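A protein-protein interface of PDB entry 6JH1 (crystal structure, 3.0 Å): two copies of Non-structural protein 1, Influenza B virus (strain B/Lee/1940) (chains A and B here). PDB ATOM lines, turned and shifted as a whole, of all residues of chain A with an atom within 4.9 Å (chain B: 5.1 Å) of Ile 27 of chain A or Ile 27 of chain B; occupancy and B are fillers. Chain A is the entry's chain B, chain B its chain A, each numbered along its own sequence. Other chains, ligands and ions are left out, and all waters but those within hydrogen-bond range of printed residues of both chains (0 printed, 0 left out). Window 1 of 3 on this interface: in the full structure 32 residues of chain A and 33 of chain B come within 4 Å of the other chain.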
ATOM      1  N   PHE A  23      37.651 -12.610 -15.831  1.00  0.00           N
ATOM      2  CA  PHE A  23      36.645 -13.493 -16.406  1.00  0.00           C
ATOM      3  C   PHE A  23      35.433 -12.696 -16.877  1.00  0.00           C
ATOM      4  O   PHE A  23      34.913 -12.914 -17.973  1.00  0.00           O
ATOM      5  CB  PHE A  23      36.205 -14.529 -15.387  1.00  0.00           C
ATOM      6  CG  PHE A  23      35.077 -15.361 -15.867  1.00  0.00           C
ATOM      7  CD1 PHE A  23      35.327 -16.457 -16.693  1.00  0.00           C
ATOM      8  CD2 PHE A  23      33.769 -15.022 -15.568  1.00  0.00           C
ATOM      9  CE1 PHE A  23      34.302 -17.216 -17.162  1.00  0.00           C
ATOM     10  CE2 PHE A  23      32.718 -15.777 -16.044  1.00  0.00           C
ATOM     11  CZ  PHE A  23      32.978 -16.863 -16.836  1.00  0.00           C
ATOM     12  N   GLU A  24      34.942 -11.784 -16.046  1.00  0.00           N
ATOM     13  CA  GLU A  24      33.788 -10.999 -16.478  1.00  0.00           C
ATOM     14  C   GLU A  24      34.149  -9.983 -17.567  1.00  0.00           C
ATOM     15  O   GLU A  24      33.265  -9.577 -18.340  1.00  0.00           O
ATOM     16  CB  GLU A  24      33.136 -10.332 -15.256  1.00  0.00           C
ATOM     17  CG  GLU A  24      33.006 -11.311 -14.077  1.00  0.00           C
ATOM     18  CD  GLU A  24      31.876 -11.018 -13.110  1.00  0.00           C
ATOM     19  OE1 GLU A  24      30.866 -11.760 -13.152  1.00  0.00           O
ATOM     20  OE2 GLU A  24      32.012 -10.081 -12.287  1.00  0.00           O
ATOM     21  N   ALA A  25      35.424  -9.580 -17.663  1.00  0.00           N
ATOM     22  CA  ALA A  25      35.860  -8.779 -18.806  1.00  0.00           C
ATOM     23  C   ALA A  25      35.669  -9.551 -20.098  1.00  0.00           C
ATOM     24  O   ALA A  25      35.072  -9.053 -21.064  1.00  0.00           O
ATOM     25  CB  ALA A  25      37.321  -8.360 -18.649  1.00  0.00           C
ATOM     26  N   GLY A  26      36.157 -10.784 -20.131  1.00  0.00           N
ATOM     27  CA  GLY A  26      35.910 -11.605 -21.301  1.00  0.00           C
ATOM     28  C   GLY A  26      34.431 -11.864 -21.529  1.00  0.00           C
ATOM     29  O   GLY A  26      33.989 -12.031 -22.670  1.00  0.00           O
ATOM     30  N   ILE A  27      33.650 -11.937 -20.453  1.00  0.00           N
ATOM     31  CA  ILE A  27      32.211 -12.074 -20.636  1.00  0.00           C
ATOM     32  C   ILE A  27      31.671 -10.893 -21.407  1.00  0.00           C
ATOM     33  O   ILE A  27      30.850 -11.043 -22.320  1.00  0.00           O
ATOM     34  CB  ILE A  27      31.514 -12.223 -19.279  1.00  0.00           C
ATOM     35  CG1 ILE A  27      31.874 -13.587 -18.708  1.00  0.00           C
ATOM     36  CG2 ILE A  27      30.022 -12.004 -19.431  1.00  0.00           C
ATOM     37  CD1 ILE A  27      31.258 -14.750 -19.478  1.00  0.00           C
ATOM     38  N   LEU A  28      32.145  -9.698 -21.060  1.00  0.00           N
ATOM     39  CA  LEU A  28      31.732  -8.488 -21.758  1.00  0.00           C
ATOM     40  C   LEU A  28      32.152  -8.533 -23.227  1.00  0.00           C
ATOM     41  O   LEU A  28      31.331  -8.310 -24.127  1.00  0.00           O
ATOM     42  CB  LEU A  28      32.306  -7.280 -21.005  1.00  0.00           C
ATOM     43  CG  LEU A  28      32.274  -5.831 -21.461  1.00  0.00           C
ATOM     44  CD1 LEU A  28      30.848  -5.327 -21.506  1.00  0.00           C
ATOM     45  CD2 LEU A  28      33.040  -5.032 -20.434  1.00  0.00           C
ATOM     46  N   GLU A  29      33.366  -8.873 -23.480  1.00  0.00           N
ATOM     47  CA  GLU A  29      33.772  -8.937 -24.831  1.00  0.00           C
ATOM     48  C   GLU A  29      32.980  -9.922 -25.631  1.00  0.00           C
ATOM     49  O   GLU A  29      32.885  -9.813 -26.797  1.00  0.00           O
ATOM     50  CB  GLU A  29      35.236  -9.231 -24.868  1.00  0.00           C
ATOM     51  CG  GLU A  29      35.775  -9.632 -26.197  1.00  0.00           C
ATOM     52  CD  GLU A  29      36.043  -8.504 -27.127  1.00  0.00           C
ATOM     53  OE1 GLU A  29      35.749  -7.367 -26.832  1.00  0.00           O
ATOM     54  OE2 GLU A  29      36.520  -8.776 -28.205  1.00  0.00           O
ATOM     55  N   CYS A  30      32.382 -10.882 -24.993  1.00  0.00           N
ATOM     56  CA  CYS A  30      31.594 -11.868 -25.676  1.00  0.00           C
ATOM     57  C   CYS A  30      30.311 -11.282 -26.060  1.00  0.00           C
ATOM     58  O   CYS A  30      29.815 -11.575 -27.072  1.00  0.00           O
ATOM     59  CB  CYS A  30      31.300 -12.988 -24.755  1.00  0.00           C
ATOM     60  SG  CYS A  30      32.185 -14.462 -25.133  1.00  0.00           S
ATOM     61  N   TYR A  31      29.764 -10.461 -25.217  1.00  0.00           N
ATOM     62  CA  TYR A  31      28.520  -9.863 -25.501  1.00  0.00           C
ATOM     63  C   TYR A  31      28.699  -8.995 -26.666  1.00  0.00           C
ATOM     64  O   TYR A  31      28.096  -9.161 -27.676  1.00  0.00           O
ATOM     65  CB  TYR A  31      28.175  -9.001 -24.354  1.00  0.00           C
ATOM     66  CG  TYR A  31      27.244  -9.598 -23.354  1.00  0.00           C
ATOM     67  CD1 TYR A  31      25.915  -9.390 -23.430  1.00  0.00           C
ATOM     68  CD2 TYR A  31      27.718 -10.318 -22.322  1.00  0.00           C
ATOM     69  CE1 TYR A  31      25.077  -9.916 -22.505  1.00  0.00           C
ATOM     70  CE2 TYR A  31      26.882 -10.832 -21.385  1.00  0.00           C
ATOM     71  CZ  TYR A  31      25.570 -10.619 -21.495  1.00  0.00           C
ATOM     72  OH  TYR A  31      24.742 -11.141 -20.571  1.00  0.00           O
ATOM     73  N   LEU A  51      27.013  -4.089 -17.136  1.00  0.00           N
ATOM     74  CA  LEU A  51      28.237  -4.850 -16.911  1.00  0.00           C
ATOM     75  C   LEU A  51      29.493  -4.014 -17.163  1.00  0.00           C
ATOM     76  O   LEU A  51      30.430  -4.033 -16.353  1.00  0.00           O
ATOM     77  CB  LEU A  51      28.240  -6.102 -17.782  1.00  0.00           C
ATOM     78  CG  LEU A  51      29.577  -6.837 -17.718  1.00  0.00           C
ATOM     79  CD1 LEU A  51      29.933  -7.281 -16.283  1.00  0.00           C
ATOM     80  CD2 LEU A  51      29.532  -8.010 -18.654  1.00  0.00           C
ATOM     81  N   MET A  85      38.307 -17.840 -21.216  1.00  0.00           N
ATOM     82  CA  MET A  85      37.076 -18.415 -21.743  1.00  0.00           C
ATOM     83  C   MET A  85      37.355 -19.570 -22.688  1.00  0.00           C
ATOM     84  O   MET A  85      36.631 -20.568 -22.684  1.00  0.00           O
ATOM     85  CB  MET A  85      36.212 -17.360 -22.396  1.00  0.00           C
ATOM     86  CG  MET A  85      35.811 -16.331 -21.395  1.00  0.00           C
ATOM     87  SD  MET A  85      34.206 -16.821 -20.822  1.00  0.00           S
ATOM     88  CE  MET A  85      33.329 -16.419 -22.306  1.00  0.00           C
ATOM     89  N   PHE B  23      22.325 -17.515 -25.592  1.00  0.00           N
ATOM     90  CA  PHE B  23      23.617 -17.003 -25.392  1.00  0.00           C
ATOM     91  C   PHE B  23      23.903 -17.022 -23.942  1.00  0.00           C
ATOM     92  O   PHE B  23      24.914 -17.472 -23.539  1.00  0.00           O
ATOM     93  CB  PHE B  23      23.627 -15.605 -25.897  1.00  0.00           C
ATOM     94  CG  PHE B  23      24.889 -14.902 -25.673  1.00  0.00           C
ATOM     95  CD1 PHE B  23      26.004 -15.301 -26.304  1.00  0.00           C
ATOM     96  CD2 PHE B  23      24.941 -13.833 -24.855  1.00  0.00           C
ATOM     97  CE1 PHE B  23      27.171 -14.660 -26.102  1.00  0.00           C
ATOM     98  CE2 PHE B  23      26.100 -13.182 -24.650  1.00  0.00           C
ATOM     99  CZ  PHE B  23      27.213 -13.603 -25.267  1.00  0.00           C
ATOM    100  N   GLU B  24      22.990 -16.537 -23.137  1.00  0.00           N
ATOM    101  CA  GLU B  24      23.216 -16.476 -21.707  1.00  0.00           C
ATOM    102  C   GLU B  24      23.269 -17.821 -21.062  1.00  0.00           C
ATOM    103  O   GLU B  24      23.877 -18.021 -20.068  1.00  0.00           O
ATOM    104  CB  GLU B  24      22.217 -15.566 -21.074  1.00  0.00           C
ATOM    105  CG  GLU B  24      22.423 -14.134 -21.497  1.00  0.00           C
ATOM    106  CD  GLU B  24      21.399 -13.189 -20.943  1.00  0.00           C
ATOM    107  OE1 GLU B  24      20.423 -13.649 -20.383  1.00  0.00           O
ATOM    108  OE2 GLU B  24      21.548 -11.985 -21.087  1.00  0.00           O
ATOM    109  N   ALA B  25      22.634 -18.773 -21.664  1.00  0.00           N
ATOM    110  CA  ALA B  25      22.693 -20.079 -21.175  1.00  0.00           C
ATOM    111  C   ALA B  25      24.145 -20.428 -21.176  1.00  0.00           C
ATOM    112  O   ALA B  25      24.624 -20.896 -20.221  1.00  0.00           O
ATOM    113  CB  ALA B  25      21.951 -20.951 -22.116  1.00  0.00           C
ATOM    114  N   GLY B  26      24.859 -20.180 -22.245  1.00  0.00           N
ATOM    115  CA  GLY B  26      26.288 -20.441 -22.293  1.00  0.00           C
ATOM    116  C   GLY B  26      27.100 -19.534 -21.380  1.00  0.00           C
ATOM    117  O   GLY B  26      28.094 -19.967 -20.794  1.00  0.00           O
ATOM    118  N   ILE B  27      26.676 -18.282 -21.199  1.00  0.00           N
ATOM    119  CA  ILE B  27      27.401 -17.453 -20.241  1.00  0.00           C
ATOM    120  C   ILE B  27      27.385 -18.117 -18.873  1.00  0.00           C
ATOM    121  O   ILE B  27      28.419 -18.221 -18.200  1.00  0.00           O
ATOM    122  CB  ILE B  27      26.801 -16.035 -20.176  1.00  0.00           C
ATOM    123  CG1 ILE B  27      27.025 -15.298 -21.494  1.00  0.00           C
ATOM    124  CG2 ILE B  27      27.409 -15.263 -19.012  1.00  0.00           C
ATOM    125  CD1 ILE B  27      28.453 -14.938 -21.781  1.00  0.00           C
ATOM    126  N   LEU B  28      26.217 -18.640 -18.480  1.00  0.00           N
ATOM    127  CA  LEU B  28      26.073 -19.325 -17.196  1.00  0.00           C
ATOM    128  C   LEU B  28      26.943 -20.572 -17.128  1.00  0.00           C
ATOM    129  O   LEU B  28      27.700 -20.763 -16.166  1.00  0.00           O
ATOM    130  CB  LEU B  28      24.602 -19.671 -16.966  1.00  0.00           C
ATOM    131  CG  LEU B  28      24.144 -20.599 -15.840  1.00  0.00           C
ATOM    132  CD1 LEU B  28      24.379 -19.957 -14.509  1.00  0.00           C
ATOM    133  CD2 LEU B  28      22.653 -20.937 -15.994  1.00  0.00           C
ATOM    134  N   GLU B  29      26.877 -21.422 -18.152  1.00  0.00           N
ATOM    135  CA  GLU B  29      27.757 -22.578 -18.154  1.00  0.00           C
ATOM    136  C   GLU B  29      29.197 -22.130 -17.934  1.00  0.00           C
ATOM    137  O   GLU B  29      29.959 -22.794 -17.227  1.00  0.00           O
ATOM    138  CB  GLU B  29      27.580 -23.365 -19.454  1.00  0.00           C
ATOM    139  CG  GLU B  29      28.469 -24.587 -19.606  1.00  0.00           C
ATOM    140  CD  GLU B  29      27.986 -25.788 -18.818  1.00  0.00           C
ATOM    141  OE1 GLU B  29      26.926 -25.688 -18.187  1.00  0.00           O
ATOM    142  OE2 GLU B  29      28.677 -26.828 -18.804  1.00  0.00           O
ATOM    143  N   CYS B  30      29.566 -20.962 -18.475  1.00  0.00           N
ATOM    144  CA  CYS B  30      30.925 -20.434 -18.305  1.00  0.00           C
ATOM    145  C   CYS B  30      31.232 -20.049 -16.866  1.00  0.00           C
ATOM    146  O   CYS B  30      32.317 -20.349 -16.357  1.00  0.00           O
ATOM    147  CB  CYS B  30      31.136 -19.236 -19.208  1.00  0.00           C
ATOM    148  SG  CYS B  30      31.746 -19.733 -20.764  1.00  0.00           S
ATOM    149  N   TYR B  31      30.298 -19.430 -16.215  1.00  0.00           N
ATOM    150  CA  TYR B  31      30.508 -19.069 -14.851  1.00  0.00           C
ATOM    151  C   TYR B  31      30.627 -20.314 -14.072  1.00  0.00           C
ATOM    152  O   TYR B  31      31.426 -20.388 -13.219  1.00  0.00           O
ATOM    153  CB  TYR B  31      29.328 -18.341 -14.311  1.00  0.00           C
ATOM    154  CG  TYR B  31      29.312 -16.871 -14.471  1.00  0.00           C
ATOM    155  CD1 TYR B  31      29.031 -16.297 -15.665  1.00  0.00           C
ATOM    156  CD2 TYR B  31      29.520 -16.071 -13.410  1.00  0.00           C
ATOM    157  CE1 TYR B  31      28.989 -14.941 -15.792  1.00  0.00           C
ATOM    158  CE2 TYR B  31      29.489 -14.724 -13.526  1.00  0.00           C
ATOM    159  CZ  TYR B  31      29.221 -14.177 -14.713  1.00  0.00           C
ATOM    160  OH  TYR B  31      29.194 -12.841 -14.783  1.00  0.00           O
ATOM    161  N   LEU B  51      21.708 -15.147 -11.997  1.00  0.00           N
ATOM    162  CA  LEU B  51      21.634 -15.440 -13.423  1.00  0.00           C
ATOM    163  C   LEU B  51      20.846 -16.726 -13.676  1.00  0.00           C
ATOM    164  O   LEU B  51      19.942 -16.755 -14.519  1.00  0.00           O
ATOM    165  CB  LEU B  51      23.047 -15.537 -14.011  1.00  0.00           C
ATOM    166  CG  LEU B  51      23.269 -15.979 -15.490  1.00  0.00           C
ATOM    167  CD1 LEU B  51      22.651 -15.011 -16.517  1.00  0.00           C
ATOM    168  CD2 LEU B  51      24.725 -16.276 -15.831  1.00  0.00           C
ATOM    169  N   MET B  85      29.257 -19.370 -28.347  1.00  0.00           N
ATOM    170  CA  MET B  85      30.415 -18.749 -27.721  1.00  0.00           C
ATOM    171  C   MET B  85      31.695 -19.169 -28.420  1.00  0.00           C
ATOM    172  O   MET B  85      32.555 -18.332 -28.695  1.00  0.00           O
ATOM    173  CB  MET B  85      30.475 -19.144 -26.262  1.00  0.00           C
ATOM    174  CG  MET B  85      29.284 -18.713 -25.492  1.00  0.00           C
ATOM    175  SD  MET B  85      29.780 -17.311 -24.582  1.00  0.00           S
ATOM    176  CE  MET B  85      30.831 -18.239 -23.497  1.00  0.00           C
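The backbone carbonyl oxygen (O) of Gly 26 of chain B sits close to the side-chain sulfur (SG) of Cys 30 of chain B, 3.7 Å away.
Glu 24 of chain A touches Tyr 31 of chain B, and with the chains exchanged Tyr 31 of chain A touches Glu 24 of chain B.
Ile 27 of chain B touches its own counterpart, Ile 27 of chain A.
Cys 30 of chain A touches Met 85 of chain B, and with the chains exchanged Met 85 of chain A touches Cys 30 of chain B.
Met 85 of chain B touches its own counterpart, Met 85 of chain A.
Of the 10 pairs that touch across the chains among the printed residues, 10 have their exchanged pair printed and touching as well.
Printed residues of chain B within 4 Å of Tyr 31 of chain A: Phe 23 and Glu 24.
Of the printed residues of chain A, Glu 24 of chain B touches Tyr 31.
Of the printed residues of chain A, Tyr 31 of chain B touches Phe 23 and Glu 24.
Of the printed residues of chain A, Cys 30 of chain B touches Phe 23 (3.6 Å) and Met 85 (3.8 Å).
Gly 26 of chain A touches none of the printed residues of chain B.
The nearest residue of chain A that does not touch Ile 27 of chain B is Tyr 31 of chain A (4.4 Å).
Of the 11 printed residues of chain A, 6 touch a printed residue of chain B.
Hydrophobic or aromatic side chains of chain A within 4 Å of the printed part of chain B: Phe 23, Ile 27, Tyr 31 and Met 85.
Among the printed residues, no Asp or Glu carboxylate lies within 4 Å of a Lys or Arg side-chain nitrogen of the other chain.
Phe 23 of chain A touches Cys 30 of chain B (CZ to O, 3.6 Å).
CE2 of Phe 23 of chain A touches CD1 of Tyr 31 of chain B, 3.7 Å away.
Ile 27 of chain A touches Ile 27 of chain B (CD1 to CD1, 3.6 Å).
Cys 30 of chain A touches Phe 23 of chain B (O to CZ, 3.8 Å).
CA of Tyr 31 of chain A touches CZ of Phe 23 of chain B, 3.97 Å away.
Met 85 of chain A touches Cys 30 of chain B.
Met 85 of chain A touches Met 85 of chain B.
OE2 of Glu 24 of chain B is in hydrogen-bond range of OH of Tyr 31 of chain A, at 3.3 Å.
The side-chain carboxylate (OE1) of Glu 24 of chain A is in hydrogen-bond range of the side-chain hydroxyl (OH) of Tyr 31 of chain B.
SD of Met 85 of chain B lies within hydrogen-bond range of SG of Cys 30 of chain A (3.8 Å).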
